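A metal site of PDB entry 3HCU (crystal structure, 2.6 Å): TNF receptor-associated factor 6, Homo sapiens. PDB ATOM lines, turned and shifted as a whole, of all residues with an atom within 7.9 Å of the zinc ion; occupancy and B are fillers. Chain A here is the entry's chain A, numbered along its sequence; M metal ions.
The zinc ion is bound by NE2 of His 102 (2.4 Å), SG of Cys 85 (2.4 Å), SG of Cys 106 (2.5 Å) and SG of Cys 90 (2.6 Å).
The zinc ion has four donor atoms within binding distance.
ND2 of Asn 87 touches the zinc ion (3.9 Å).
SG of Cys 106 lies close to ND2 of Asn 87 (3.1 Å).
ND2 of Asn 87 sits at hydrogen-bond distance from O of Phe 108 (3.5 Å).
SG of Cys 106 sits close to O of Phe 108.
The side-chain sulfur (SG) of Cys 90 sits close to the backbone NH (N) of His 92, 3.1 Å away.
NE2 of Gln 103 sits close to ND2 of Asn 87.
SG of Cys 85 lies close to ND2 of Asn 87.
O of His 92 sits at hydrogen-bond distance from N of Cys 85.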
ATOM      1  N   LYS A  84       9.540   9.347  -4.758  1.00  0.00           N
ATOM      2  CA  LYS A  84      10.993   9.491  -4.837  1.00  0.00           C
ATOM      3  C   LYS A  84      11.367  10.902  -4.455  1.00  0.00           C
ATOM      4  O   LYS A  84      10.609  11.836  -4.684  1.00  0.00           O
ATOM      5  CB  LYS A  84      11.492   9.216  -6.274  1.00  0.00           C
ATOM      6  CG  LYS A  84      12.939   9.738  -6.543  1.00  0.00           C
ATOM      7  CD  LYS A  84      13.415   9.496  -7.975  1.00  0.00           C
ATOM      8  CE  LYS A  84      12.479  10.121  -8.998  1.00  0.00           C
ATOM      9  NZ  LYS A  84      12.996  10.014 -10.385  1.00  0.00           N
ATOM     10  N   CYS A  85      12.548  11.073  -3.874  1.00  0.00           N
ATOM     11  CA  CYS A  85      12.962  12.399  -3.480  1.00  0.00           C
ATOM     12  C   CYS A  85      13.017  13.302  -4.717  1.00  0.00           C
ATOM     13  O   CYS A  85      13.607  12.949  -5.744  1.00  0.00           O
ATOM     14  CB  CYS A  85      14.321  12.357  -2.796  1.00  0.00           C
ATOM     15  SG  CYS A  85      14.546  13.789  -1.742  1.00  0.00           S
ATOM     16  N   PRO A  86      12.382  14.474  -4.643  1.00  0.00           N
ATOM     17  CA  PRO A  86      12.397  15.382  -5.783  1.00  0.00           C
ATOM     18  C   PRO A  86      13.570  16.361  -5.778  1.00  0.00           C
ATOM     19  O   PRO A  86      13.471  17.455  -6.339  1.00  0.00           O
ATOM     20  CB  PRO A  86      11.056  16.085  -5.657  1.00  0.00           C
ATOM     21  CG  PRO A  86      10.944  16.254  -4.170  1.00  0.00           C
ATOM     22  CD  PRO A  86      11.421  14.914  -3.622  1.00  0.00           C
ATOM     23  N   ASN A  87      14.677  15.958  -5.155  1.00  0.00           N
ATOM     24  CA  ASN A  87      15.868  16.803  -5.078  1.00  0.00           C
ATOM     25  C   ASN A  87      16.875  16.551  -6.184  1.00  0.00           C
ATOM     26  O   ASN A  87      18.025  16.955  -6.093  1.00  0.00           O
ATOM     27  CB  ASN A  87      16.551  16.654  -3.717  1.00  0.00           C
ATOM     28  CG  ASN A  87      15.777  17.335  -2.609  1.00  0.00           C
ATOM     29  OD1 ASN A  87      15.356  18.492  -2.752  1.00  0.00           O
ATOM     30  ND2 ASN A  87      15.581  16.634  -1.497  1.00  0.00           N
ATOM     31  N   GLU A  88      16.413  15.870  -7.233  1.00  0.00           N
ATOM     32  CA  GLU A  88      17.246  15.579  -8.392  1.00  0.00           C
ATOM     33  C   GLU A  88      18.671  15.164  -8.028  1.00  0.00           C
ATOM     34  O   GLU A  88      19.507  15.980  -7.618  1.00  0.00           O
ATOM     35  CB  GLU A  88      17.269  16.790  -9.323  1.00  0.00           C
ATOM     36  CG  GLU A  88      17.597  16.433 -10.752  1.00  0.00           C
ATOM     37  CD  GLU A  88      17.540  17.612 -11.684  1.00  0.00           C
ATOM     38  OE1 GLU A  88      17.674  17.397 -12.907  1.00  0.00           O
ATOM     39  OE2 GLU A  88      17.350  18.753 -11.198  1.00  0.00           O
ATOM     40  N   GLY A  89      18.956  13.877  -8.198  1.00  0.00           N
ATOM     41  CA  GLY A  89      20.261  13.356  -7.855  1.00  0.00           C
ATOM     42  C   GLY A  89      20.033  12.350  -6.749  1.00  0.00           C
ATOM     43  O   GLY A  89      20.573  11.246  -6.789  1.00  0.00           O
ATOM     44  N   CYS A  90      19.222  12.730  -5.764  1.00  0.00           N
ATOM     45  CA  CYS A  90      18.942  11.811  -4.673  1.00  0.00           C
ATOM     46  C   CYS A  90      18.166  10.644  -5.239  1.00  0.00           C
ATOM     47  O   CYS A  90      17.367  10.810  -6.159  1.00  0.00           O
ATOM     48  CB  CYS A  90      18.122  12.447  -3.564  1.00  0.00           C
ATOM     49  SG  CYS A  90      17.632  11.174  -2.366  1.00  0.00           S
ATOM     50  N   LEU A  91      18.374   9.473  -4.635  1.00  0.00           N
ATOM     51  CA  LEU A  91      17.735   8.253  -5.089  1.00  0.00           C
ATOM     52  C   LEU A  91      16.948   7.578  -3.964  1.00  0.00           C
ATOM     53  O   LEU A  91      16.813   6.351  -3.939  1.00  0.00           O
ATOM     54  CB  LEU A  91      18.814   7.321  -5.667  1.00  0.00           C
ATOM     55  CG  LEU A  91      19.835   8.055  -6.567  1.00  0.00           C
ATOM     56  CD1 LEU A  91      21.196   7.389  -6.483  1.00  0.00           C
ATOM     57  CD2 LEU A  91      19.331   8.148  -8.004  1.00  0.00           C
ATOM     58  N   HIS A  92      16.430   8.394  -3.056  1.00  0.00           N
ATOM     59  CA  HIS A  92      15.640   7.901  -1.918  1.00  0.00           C
ATOM     60  C   HIS A  92      14.157   7.765  -2.256  1.00  0.00           C
ATOM     61  O   HIS A  92      13.601   8.566  -3.003  1.00  0.00           O
ATOM     62  CB  HIS A  92      15.794   8.862  -0.723  1.00  0.00           C
ATOM     63  CG  HIS A  92      16.815   8.418   0.276  1.00  0.00           C
ATOM     64  ND1 HIS A  92      16.586   7.400   1.185  1.00  0.00           N
ATOM     65  CD2 HIS A  92      18.061   8.876   0.539  1.00  0.00           C
ATOM     66  CE1 HIS A  92      17.644   7.258   1.962  1.00  0.00           C
ATOM     67  NE2 HIS A  92      18.557   8.135   1.594  1.00  0.00           N
ATOM     68  N   LYS A  93      13.523   6.741  -1.695  1.00  0.00           N
ATOM     69  CA  LYS A  93      12.101   6.506  -1.918  1.00  0.00           C
ATOM     70  C   LYS A  93      11.424   6.123  -0.597  1.00  0.00           C
ATOM     71  O   LYS A  93      11.986   5.342   0.181  1.00  0.00           O
ATOM     72  CB  LYS A  93      11.890   5.415  -2.985  1.00  0.00           C
ATOM     73  CG  LYS A  93      12.330   4.017  -2.576  1.00  0.00           C
ATOM     74  CD  LYS A  93      11.882   2.936  -3.585  1.00  0.00           C
ATOM     75  CE  LYS A  93      12.336   1.525  -3.183  1.00  0.00           C
ATOM     76  NZ  LYS A  93      11.895   1.134  -1.799  1.00  0.00           N
ATOM     77  N   MET A  94      10.243   6.685  -0.343  1.00  0.00           N
ATOM     78  CA  MET A  94       9.484   6.396   0.892  1.00  0.00           C
ATOM     79  C   MET A  94       8.011   6.776   0.749  1.00  0.00           C
ATOM     80  O   MET A  94       7.593   7.296  -0.298  1.00  0.00           O
ATOM     81  CB  MET A  94      10.064   7.191   2.062  1.00  0.00           C
ATOM     82  CG  MET A  94       9.582   8.615   2.100  1.00  0.00           C
ATOM     83  SD  MET A  94      10.930   9.759   2.208  1.00  0.00           S
ATOM     84  CE  MET A  94      11.481   9.756   0.516  1.00  0.00           C
ATOM     85  N   LEU A  99       8.063  11.987   3.196  1.00  0.00           N
ATOM     86  CA  LEU A  99       8.994  12.743   2.375  1.00  0.00           C
ATOM     87  C   LEU A  99       9.574  13.923   3.136  1.00  0.00           C
ATOM     88  O   LEU A  99      10.783  14.052   3.278  1.00  0.00           O
ATOM     89  CB  LEU A  99       8.291  13.252   1.113  1.00  0.00           C
ATOM     90  CG  LEU A  99       9.198  14.119   0.226  1.00  0.00           C
ATOM     91  CD1 LEU A  99      10.501  13.389  -0.043  1.00  0.00           C
ATOM     92  CD2 LEU A  99       8.492  14.416  -1.090  1.00  0.00           C
ATOM     93  N   HIS A 102      12.280  13.258   5.670  1.00  0.00           N
ATOM     94  CA  HIS A 102      13.512  12.910   4.979  1.00  0.00           C
ATOM     95  C   HIS A 102      14.276  14.175   4.539  1.00  0.00           C
ATOM     96  O   HIS A 102      15.497  14.209   4.596  1.00  0.00           O
ATOM     97  CB  HIS A 102      13.190  12.066   3.753  1.00  0.00           C
ATOM     98  CG  HIS A 102      14.342  11.919   2.811  1.00  0.00           C
ATOM     99  ND1 HIS A 102      15.455  11.157   3.091  1.00  0.00           N
ATOM    100  CD2 HIS A 102      14.565  12.477   1.593  1.00  0.00           C
ATOM    101  CE1 HIS A 102      16.314  11.253   2.095  1.00  0.00           C
ATOM    102  NE2 HIS A 102      15.797  12.045   1.168  1.00  0.00           N
ATOM    103  N   GLN A 103      13.550  15.192   4.108  1.00  0.00           N
ATOM    104  CA  GLN A 103      14.161  16.441   3.641  1.00  0.00           C
ATOM    105  C   GLN A 103      15.217  16.991   4.592  1.00  0.00           C
ATOM    106  O   GLN A 103      16.278  17.452   4.164  1.00  0.00           O
ATOM    107  CB  GLN A 103      13.095  17.516   3.446  1.00  0.00           C
ATOM    108  CG  GLN A 103      13.517  18.620   2.501  1.00  0.00           C
ATOM    109  CD  GLN A 103      13.820  18.080   1.127  1.00  0.00           C
ATOM    110  OE1 GLN A 103      13.038  17.296   0.576  1.00  0.00           O
ATOM    111  NE2 GLN A 103      14.944  18.477   0.563  1.00  0.00           N
ATOM    112  N   HIS A 105      17.256  15.632   6.062  1.00  0.00           N
ATOM    113  CA  HIS A 105      18.441  14.793   5.997  1.00  0.00           C
ATOM    114  C   HIS A 105      18.887  14.469   4.556  1.00  0.00           C
ATOM    115  O   HIS A 105      19.483  13.414   4.309  1.00  0.00           O
ATOM    116  CB  HIS A 105      18.146  13.462   6.722  1.00  0.00           C
ATOM    117  CG  HIS A 105      17.629  13.620   8.125  1.00  0.00           C
ATOM    118  ND1 HIS A 105      17.138  12.555   8.850  1.00  0.00           N
ATOM    119  CD2 HIS A 105      17.547  14.694   8.941  1.00  0.00           C
ATOM    120  CE1 HIS A 105      16.798  12.964  10.050  1.00  0.00           C
ATOM    121  NE2 HIS A 105      17.031  14.264  10.132  1.00  0.00           N
ATOM    122  N   CYS A 106      18.600  15.351   3.596  1.00  0.00           N
ATOM    123  CA  CYS A 106      18.987  15.074   2.211  1.00  0.00           C
ATOM    124  C   CYS A 106      20.391  15.564   1.861  1.00  0.00           C
ATOM    125  O   CYS A 106      20.834  16.611   2.347  1.00  0.00           O
ATOM    126  CB  CYS A 106      17.973  15.680   1.226  1.00  0.00           C
ATOM    127  SG  CYS A 106      17.995  14.980  -0.470  1.00  0.00           S
ATOM    128  N   GLU A 107      21.075  14.799   1.027  1.00  0.00           N
ATOM    129  CA  GLU A 107      22.429  15.158   0.606  1.00  0.00           C
ATOM    130  C   GLU A 107      22.304  16.292  -0.401  1.00  0.00           C
ATOM    131  O   GLU A 107      23.200  17.116  -0.537  1.00  0.00           O
ATOM    132  CB  GLU A 107      23.099  13.955  -0.043  1.00  0.00           C
ATOM    133  CG  GLU A 107      22.860  12.645   0.720  1.00  0.00           C
ATOM    134  CD  GLU A 107      23.071  12.795   2.224  1.00  0.00           C
ATOM    135  OE1 GLU A 107      24.195  13.121   2.643  1.00  0.00           O
ATOM    136  OE2 GLU A 107      22.095  12.584   2.978  1.00  0.00           O
ATOM    137  N   PHE A 108      21.168  16.316  -1.087  1.00  0.00           N
ATOM    138  CA  PHE A 108      20.914  17.342  -2.066  1.00  0.00           C
ATOM    139  C   PHE A 108      19.835  18.230  -1.457  1.00  0.00           C
ATOM    140  O   PHE A 108      18.829  17.725  -0.979  1.00  0.00           O
ATOM    141  CB  PHE A 108      20.428  16.711  -3.363  1.00  0.00           C
ATOM    142  CG  PHE A 108      21.262  15.549  -3.826  1.00  0.00           C
ATOM    143  CD1 PHE A 108      21.215  14.337  -3.159  1.00  0.00           C
ATOM    144  CD2 PHE A 108      22.081  15.663  -4.942  1.00  0.00           C
ATOM    145  CE1 PHE A 108      21.987  13.249  -3.597  1.00  0.00           C
ATOM    146  CE2 PHE A 108      22.855  14.581  -5.388  1.00  0.00           C
ATOM    147  CZ  PHE A 108      22.801  13.375  -4.717  1.00  0.00           C
ATOM    148  N   ALA A 109      20.032  19.553  -1.435  1.00  0.00           N
ATOM    149  CA  ALA A 109      19.023  20.411  -0.839  1.00  0.00           C
ATOM    150  C   ALA A 109      19.278  21.921  -0.846  1.00  0.00           C
ATOM    151  O   ALA A 109      19.642  22.498  -1.851  1.00  0.00           O
ATOM    152  CB  ALA A 109      18.741  19.935   0.584  1.00  0.00           C
HETATM  153 ZN    ZN M   1      16.619  12.981  -0.840  1.00  0.00          ZN
